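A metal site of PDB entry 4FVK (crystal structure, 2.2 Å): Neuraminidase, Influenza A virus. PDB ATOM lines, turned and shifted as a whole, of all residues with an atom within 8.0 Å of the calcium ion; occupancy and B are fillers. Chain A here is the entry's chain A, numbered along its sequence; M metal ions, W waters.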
ATOM      1  N   ASN A 199      -5.399  -7.816  27.069  1.00  0.00           N
ATOM      2  CA  ASN A 199      -4.737  -9.092  26.943  1.00  0.00           C
ATOM      3  C   ASN A 199      -3.380  -8.939  27.615  1.00  0.00           C
ATOM      4  O   ASN A 199      -2.741  -7.899  27.497  1.00  0.00           O
ATOM      5  CB  ASN A 199      -4.650  -9.456  25.458  1.00  0.00           C
ATOM      6  CG  ASN A 199      -3.703 -10.614  25.192  1.00  0.00           C
ATOM      7  OD1 ASN A 199      -2.660 -10.438  24.549  1.00  0.00           O
ATOM      8  ND2 ASN A 199      -4.069 -11.797  25.661  1.00  0.00           N
ATOM      9  N   GLY A 216       3.375  -6.872  30.957  1.00  0.00           N
ATOM     10  CA  GLY A 216       2.748  -7.781  30.032  1.00  0.00           C
ATOM     11  C   GLY A 216       2.923  -7.384  28.573  1.00  0.00           C
ATOM     12  O   GLY A 216       3.516  -6.359  28.254  1.00  0.00           O
ATOM     13  N   THR A 217       2.447  -8.239  27.690  1.00  0.00           N
ATOM     14  CA  THR A 217       2.401  -7.918  26.270  1.00  0.00           C
ATOM     15  C   THR A 217       0.919  -8.066  25.895  1.00  0.00           C
ATOM     16  O   THR A 217       0.332  -9.128  26.137  1.00  0.00           O
ATOM     17  CB  THR A 217       3.290  -8.878  25.445  1.00  0.00           C
ATOM     18  OG1 THR A 217       4.683  -8.713  25.807  1.00  0.00           O
ATOM     19  CG2 THR A 217       3.155  -8.606  23.956  1.00  0.00           C
ATOM     20  N   ASN A 218       0.315  -7.011  25.366  1.00  0.00           N
ATOM     21  CA  ASN A 218      -1.062  -7.065  24.877  1.00  0.00           C
ATOM     22  C   ASN A 218      -1.042  -7.406  23.398  1.00  0.00           C
ATOM     23  O   ASN A 218      -0.678  -6.574  22.575  1.00  0.00           O
ATOM     24  CB  ASN A 218      -1.775  -5.711  25.106  1.00  0.00           C
ATOM     25  CG  ASN A 218      -3.265  -5.781  24.815  1.00  0.00           C
ATOM     26  OD1 ASN A 218      -3.718  -6.391  23.833  1.00  0.00           O
ATOM     27  ND2 ASN A 218      -4.045  -5.147  25.667  1.00  0.00           N
ATOM     28  N   LEU A 219      -1.423  -8.640  23.068  1.00  0.00           N
ATOM     29  CA  LEU A 219      -1.415  -9.074  21.676  1.00  0.00           C
ATOM     30  C   LEU A 219      -2.718  -8.711  20.937  1.00  0.00           C
ATOM     31  O   LEU A 219      -2.816  -8.918  19.725  1.00  0.00           O
ATOM     32  CB  LEU A 219      -1.179 -10.589  21.595  1.00  0.00           C
ATOM     33  CG  LEU A 219       0.157 -11.149  22.099  1.00  0.00           C
ATOM     34  CD1 LEU A 219       0.150 -12.656  22.000  1.00  0.00           C
ATOM     35  CD2 LEU A 219       1.323 -10.587  21.310  1.00  0.00           C
ATOM     36  N   TRP A 220      -3.681  -8.152  21.668  1.00  0.00           N
ATOM     37  CA  TRP A 220      -5.019  -7.858  21.155  1.00  0.00           C
ATOM     38  C   TRP A 220      -5.189  -6.394  20.689  1.00  0.00           C
ATOM     39  O   TRP A 220      -5.352  -6.147  19.502  1.00  0.00           O
ATOM     40  CB  TRP A 220      -6.076  -8.218  22.213  1.00  0.00           C
ATOM     41  CG  TRP A 220      -7.511  -7.861  21.892  1.00  0.00           C
ATOM     42  CD1 TRP A 220      -8.051  -7.623  20.654  1.00  0.00           C
ATOM     43  CD2 TRP A 220      -8.582  -7.694  22.840  1.00  0.00           C
ATOM     44  NE1 TRP A 220      -9.382  -7.307  20.780  1.00  0.00           N
ATOM     45  CE2 TRP A 220      -9.734  -7.340  22.106  1.00  0.00           C
ATOM     46  CE3 TRP A 220      -8.665  -7.797  24.230  1.00  0.00           C
ATOM     47  CZ2 TRP A 220     -10.962  -7.115  22.714  1.00  0.00           C
ATOM     48  CZ3 TRP A 220      -9.892  -7.571  24.838  1.00  0.00           C
ATOM     49  CH2 TRP A 220     -11.026  -7.233  24.076  1.00  0.00           C
ATOM     50  N   ASN A 221      -5.125  -5.444  21.613  1.00  0.00           N
ATOM     51  CA  ASN A 221      -5.502  -4.062  21.298  1.00  0.00           C
ATOM     52  C   ASN A 221      -4.655  -2.944  21.882  1.00  0.00           C
ATOM     53  O   ASN A 221      -5.186  -1.885  22.209  1.00  0.00           O
ATOM     54  CB  ASN A 221      -6.956  -3.833  21.738  1.00  0.00           C
ATOM     55  CG  ASN A 221      -7.167  -4.149  23.220  1.00  0.00           C
ATOM     56  OD1 ASN A 221      -6.195  -4.385  23.960  1.00  0.00           O
ATOM     57  ND2 ASN A 221      -8.414  -4.166  23.655  1.00  0.00           N
ATOM     58  N   ASP A 222      -3.345  -3.144  22.037  1.00  0.00           N
ATOM     59  CA  ASP A 222      -2.542  -2.125  22.708  1.00  0.00           C
ATOM     60  C   ASP A 222      -1.069  -2.253  22.301  1.00  0.00           C
ATOM     61  O   ASP A 222      -0.510  -3.357  22.280  1.00  0.00           O
ATOM     62  CB  ASP A 222      -2.736  -2.248  24.216  1.00  0.00           C
ATOM     63  CG  ASP A 222      -2.332  -1.009  24.979  1.00  0.00           C
ATOM     64  OD1 ASP A 222      -1.934  -0.007  24.364  1.00  0.00           O
ATOM     65  OD2 ASP A 222      -2.423  -1.028  26.221  1.00  0.00           O
ATOM     66  N   ALA A 223      -0.463  -1.107  21.993  1.00  0.00           N
ATOM     67  CA  ALA A 223       0.952  -1.044  21.680  1.00  0.00           C
ATOM     68  C   ALA A 223       1.704  -0.519  22.888  1.00  0.00           C
ATOM     69  O   ALA A 223       2.929  -0.467  22.881  1.00  0.00           O
ATOM     70  CB  ALA A 223       1.194  -0.143  20.466  1.00  0.00           C
ATOM     71  N   LYS A 224       0.962  -0.065  23.905  1.00  0.00           N
ATOM     72  CA  LYS A 224       1.570   0.158  25.211  1.00  0.00           C
ATOM     73  C   LYS A 224       1.530  -1.188  25.882  1.00  0.00           C
ATOM     74  O   LYS A 224       0.796  -2.063  25.443  1.00  0.00           O
ATOM     75  CB  LYS A 224       0.771   1.162  26.044  1.00  0.00           C
ATOM     76  CG  LYS A 224       1.126   2.649  25.804  1.00  0.00           C
ATOM     77  CD  LYS A 224       0.142   3.532  26.581  1.00  0.00           C
ATOM     78  CE  LYS A 224       0.305   5.012  26.275  1.00  0.00           C
ATOM     79  NZ  LYS A 224      -0.631   5.789  27.121  1.00  0.00           N
ATOM     80  N   ARG A 225       2.288  -1.337  26.959  1.00  0.00           N
ATOM     81  CA  ARG A 225       2.419  -2.581  27.688  1.00  0.00           C
ATOM     82  C   ARG A 225       1.667  -2.423  28.988  1.00  0.00           C
ATOM     83  O   ARG A 225       1.911  -1.482  29.717  1.00  0.00           O
ATOM     84  CB  ARG A 225       3.901  -2.855  28.014  1.00  0.00           C
ATOM     85  CG  ARG A 225       4.747  -3.138  26.797  1.00  0.00           C
ATOM     86  CD  ARG A 225       6.185  -3.677  27.162  1.00  0.00           C
ATOM     87  NE  ARG A 225       6.903  -4.037  25.946  1.00  0.00           N
ATOM     88  CZ  ARG A 225       6.684  -5.154  25.261  1.00  0.00           C
ATOM     89  NH1 ARG A 225       5.795  -6.039  25.711  1.00  0.00           N
ATOM     90  NH2 ARG A 225       7.361  -5.386  24.145  1.00  0.00           N
ATOM     91  N   PRO A 226       0.756  -3.355  29.290  1.00  0.00           N
ATOM     92  CA  PRO A 226       0.083  -3.264  30.588  1.00  0.00           C
ATOM     93  C   PRO A 226       0.985  -3.703  31.731  1.00  0.00           C
ATOM     94  O   PRO A 226       1.898  -4.502  31.538  1.00  0.00           O
ATOM     95  CB  PRO A 226      -1.115  -4.201  30.430  1.00  0.00           C
ATOM     96  CG  PRO A 226      -0.777  -5.084  29.263  1.00  0.00           C
ATOM     97  CD  PRO A 226       0.052  -4.239  28.352  1.00  0.00           C
ATOM     98  N   THR A 247       5.644   0.944  23.811  1.00  0.00           N
ATOM     99  CA  THR A 247       6.896   0.189  23.755  1.00  0.00           C
ATOM    100  C   THR A 247       6.809  -1.214  23.155  1.00  0.00           C
ATOM    101  O   THR A 247       7.808  -1.909  23.086  1.00  0.00           O
ATOM    102  CB  THR A 247       7.606   0.122  25.136  1.00  0.00           C
ATOM    103  OG1 THR A 247       6.816  -0.617  26.070  1.00  0.00           O
ATOM    104  CG2 THR A 247       7.867   1.515  25.652  1.00  0.00           C
ATOM    105  N   ASP A 248       5.616  -1.618  22.737  1.00  0.00           N
ATOM    106  CA  ASP A 248       5.470  -2.920  22.107  1.00  0.00           C
ATOM    107  C   ASP A 248       6.077  -2.850  20.716  1.00  0.00           C
ATOM    108  O   ASP A 248       6.480  -1.786  20.268  1.00  0.00           O
ATOM    109  CB  ASP A 248       3.988  -3.312  22.042  1.00  0.00           C
ATOM    110  CG  ASP A 248       3.766  -4.816  21.977  1.00  0.00           C
ATOM    111  OD1 ASP A 248       4.773  -5.573  21.913  1.00  0.00           O
ATOM    112  OD2 ASP A 248       2.589  -5.244  21.993  1.00  0.00           O
ATOM    113  N   PHE A 249       6.198  -3.992  20.063  1.00  0.00           N
ATOM    114  CA  PHE A 249       6.441  -4.017  18.627  1.00  0.00           C
ATOM    115  C   PHE A 249       5.522  -5.076  18.086  1.00  0.00           C
ATOM    116  O   PHE A 249       5.555  -6.193  18.582  1.00  0.00           O
ATOM    117  CB  PHE A 249       7.905  -4.336  18.244  1.00  0.00           C
ATOM    118  CG  PHE A 249       8.153  -4.190  16.776  1.00  0.00           C
ATOM    119  CD1 PHE A 249       8.599  -2.975  16.257  1.00  0.00           C
ATOM    120  CD2 PHE A 249       7.820  -5.206  15.889  1.00  0.00           C
ATOM    121  CE1 PHE A 249       8.774  -2.818  14.887  1.00  0.00           C
ATOM    122  CE2 PHE A 249       7.984  -5.046  14.527  1.00  0.00           C
ATOM    123  CZ  PHE A 249       8.465  -3.858  14.022  1.00  0.00           C
ATOM    124  N   PRO A 250       4.686  -4.732  17.092  1.00  0.00           N
ATOM    125  CA  PRO A 250       4.553  -3.445  16.390  1.00  0.00           C
ATOM    126  C   PRO A 250       3.973  -2.310  17.241  1.00  0.00           C
ATOM    127  O   PRO A 250       3.392  -2.530  18.293  1.00  0.00           O
ATOM    128  CB  PRO A 250       3.559  -3.772  15.281  1.00  0.00           C
ATOM    129  CG  PRO A 250       2.706  -4.808  15.864  1.00  0.00           C
ATOM    130  CD  PRO A 250       3.681  -5.699  16.602  1.00  0.00           C
ATOM    131  N   ARG A 251       4.134  -1.088  16.744  1.00  0.00           N
ATOM    132  CA  ARG A 251       3.546   0.064  17.382  1.00  0.00           C
ATOM    133  C   ARG A 251       3.448   1.201  16.381  1.00  0.00           C
ATOM    134  O   ARG A 251       4.001   1.117  15.281  1.00  0.00           O
ATOM    135  CB  ARG A 251       4.382   0.492  18.599  1.00  0.00           C
ATOM    136  CG  ARG A 251       5.756   1.021  18.251  1.00  0.00           C
ATOM    137  CD  ARG A 251       6.507   1.488  19.493  1.00  0.00           C
ATOM    138  NE  ARG A 251       7.863   1.931  19.180  1.00  0.00           N
ATOM    139  CZ  ARG A 251       8.919   1.112  19.112  1.00  0.00           C
ATOM    140  NH1 ARG A 251       8.766  -0.181  19.335  1.00  0.00           N
ATOM    141  NH2 ARG A 251      10.119   1.598  18.821  1.00  0.00           N
ATOM    142  N   ALA A 262      -2.807   2.772  23.729  1.00  0.00           N
ATOM    143  CA  ALA A 262      -2.478   3.143  22.357  1.00  0.00           C
ATOM    144  C   ALA A 262      -2.868   1.995  21.458  1.00  0.00           C
ATOM    145  O   ALA A 262      -2.230   0.938  21.476  1.00  0.00           O
ATOM    146  CB  ALA A 262      -1.000   3.422  22.240  1.00  0.00           C
ATOM    147  N   GLN A 263      -3.907   2.178  20.650  1.00  0.00           N
ATOM    148  CA  GLN A 263      -4.468   1.072  19.883  1.00  0.00           C
ATOM    149  C   GLN A 263      -4.020   0.994  18.417  1.00  0.00           C
ATOM    150  O   GLN A 263      -4.240  -0.018  17.764  1.00  0.00           O
ATOM    151  CB  GLN A 263      -5.989   1.099  20.015  1.00  0.00           C
ATOM    152  CG  GLN A 263      -6.443   1.298  21.451  1.00  0.00           C
ATOM    153  CD  GLN A 263      -7.745   0.609  21.754  1.00  0.00           C
ATOM    154  OE1 GLN A 263      -8.064  -0.420  21.169  1.00  0.00           O
ATOM    155  NE2 GLN A 263      -8.512   1.173  22.682  1.00  0.00           N
ATOM    156  N   GLU A 264      -3.382   2.049  17.927  1.00  0.00           N
ATOM    157  CA  GLU A 264      -2.777   2.022  16.603  1.00  0.00           C
ATOM    158  C   GLU A 264      -1.746   0.872  16.559  1.00  0.00           C
ATOM    159  O   GLU A 264      -0.771   0.873  17.331  1.00  0.00           O
ATOM    160  CB  GLU A 264      -2.117   3.380  16.281  1.00  0.00           C
ATOM    161  CG  GLU A 264      -1.834   3.651  14.794  1.00  0.00           C
ATOM    162  CD  GLU A 264      -1.185   5.028  14.561  1.00  0.00           C
ATOM    163  OE1 GLU A 264      -0.081   5.263  15.098  1.00  0.00           O
ATOM    164  OE2 GLU A 264      -1.771   5.873  13.838  1.00  0.00           O
ATOM    165  N   LYS A 265      -1.968  -0.094  15.682  1.00  0.00           N
ATOM    166  CA  LYS A 265      -1.077  -1.241  15.563  1.00  0.00           C
ATOM    167  C   LYS A 265      -0.971  -2.010  16.878  1.00  0.00           C
ATOM    168  O   LYS A 265       0.083  -2.548  17.181  1.00  0.00           O
ATOM    169  CB  LYS A 265       0.334  -0.808  15.122  1.00  0.00           C
ATOM    170  CG  LYS A 265       0.424   0.091  13.884  1.00  0.00           C
ATOM    171  CD  LYS A 265       0.620  -0.711  12.596  1.00  0.00           C
ATOM    172  CE  LYS A 265      -0.710  -1.269  12.055  1.00  0.00           C
ATOM    173  NZ  LYS A 265      -0.520  -2.348  11.038  1.00  0.00           N
ATOM    174  N   GLY A 266      -2.046  -2.058  17.662  1.00  0.00           N
ATOM    175  CA  GLY A 266      -2.016  -2.754  18.938  1.00  0.00           C
ATOM    176  C   GLY A 266      -2.032  -4.263  18.800  1.00  0.00           C
ATOM    177  O   GLY A 266      -1.697  -4.992  19.727  1.00  0.00           O
ATOM    178  N   GLU A 267      -2.430  -4.744  17.620  1.00  0.00           N
ATOM    179  CA  GLU A 267      -2.535  -6.161  17.371  1.00  0.00           C
ATOM    180  C   GLU A 267      -1.141  -6.773  17.279  1.00  0.00           C
ATOM    181  O   GLU A 267      -0.244  -6.187  16.670  1.00  0.00           O
ATOM    182  CB  GLU A 267      -3.312  -6.411  16.082  1.00  0.00           C
ATOM    183  CG  GLU A 267      -4.013  -7.757  16.021  1.00  0.00           C
ATOM    184  CD  GLU A 267      -4.691  -7.990  14.673  1.00  0.00           C
ATOM    185  OE1 GLU A 267      -4.887  -9.172  14.304  1.00  0.00           O
ATOM    186  OE2 GLU A 267      -5.037  -6.996  13.997  1.00  0.00           O
ATOM    187  N   GLY A 268      -0.971  -7.953  17.863  1.00  0.00           N
ATOM    188  CA  GLY A 268       0.332  -8.578  17.909  1.00  0.00           C
ATOM    189  C   GLY A 268       1.196  -7.932  18.971  1.00  0.00           C
ATOM    190  O   GLY A 268       0.719  -7.118  19.768  1.00  0.00           O
ATOM    191  N   GLY A 269       2.482  -8.290  18.987  1.00  0.00           N
ATOM    192  CA  GLY A 269       3.400  -7.801  20.001  1.00  0.00           C
ATOM    193  C   GLY A 269       4.561  -8.729  20.286  1.00  0.00           C
ATOM    194  O   GLY A 269       4.722  -9.766  19.656  1.00  0.00           O
ATOM    195  N   ILE A 270       5.387  -8.359  21.247  1.00  0.00           N
ATOM    196  CA  ILE A 270       6.558  -9.174  21.564  1.00  0.00           C
ATOM    197  C   ILE A 270       6.849  -8.968  23.032  1.00  0.00           C
ATOM    198  O   ILE A 270       6.656  -7.861  23.556  1.00  0.00           O
ATOM    199  CB  ILE A 270       7.761  -8.773  20.637  1.00  0.00           C
ATOM    200  CG1 ILE A 270       8.895  -9.781  20.717  1.00  0.00           C
ATOM    201  CG2 ILE A 270       8.281  -7.354  20.939  1.00  0.00           C
ATOM    202  CD1 ILE A 270       9.866  -9.626  19.551  1.00  0.00           C
HETATM  203 CA    CA M   1       0.432  -5.209  21.122  1.00  0.00          CA
HETATM  204  O   HOH W   1       1.343  -3.837  19.352  1.00  0.00           O
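Five residues have an atom within 4 Å of the calcium ion: Asn 218, Asp 222, Asp 248, Gly 266 and Gly 268.
The nearest printed residue that does not touch the calcium ion is Gly 269 (4.1 Å).
The backbone NH of Trp 220 sits at hydrogen-bond distance from the side-chain amide oxygen of Asn 218 (2.8 Å).
The backbone NH (N) of Asn 221 sits at hydrogen-bond distance from the side-chain amide oxygen (OD1) of Asn 218 (2.8 Å).
The backbone NH of Asn 199 lies close to the side-chain amide nitrogen of Asn 218.
NH1 of Arg 251 sits at hydrogen-bond distance from O of Asp 248.
The side-chain carboxylate of Asp 248 lies within salt-bridge range of the guanidinium group of Arg 225 (3.4 Å).
N of Gly 268 is in hydrogen-bond range of O of Leu 219 (2.8 Å).
The side-chain carboxylate (OD1) of Asp 222 is in hydrogen-bond range of the backbone NH (N) of Lys 224, at 2.9 Å.
The backbone NH (N) of Ala 262 is in hydrogen-bond range of the side-chain carboxylate (OD1) of Asp 222 (3.0 Å).
Water W1 lies within hydrogen-bond range of O of Pro 250 (2.7 Å) and O of Lys 265 (2.8 Å).
The calcium ion is bound by O of Asn 218 (2.3 Å), OD2 of Asp 248 (2.3 Å), O of Gly 268 (2.4 Å), O of Asp 222 (2.4 Å), water W1 (2.4 Å) and O of Gly 266 (2.6 Å).
The calcium ion has six donor atoms within binding distance.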
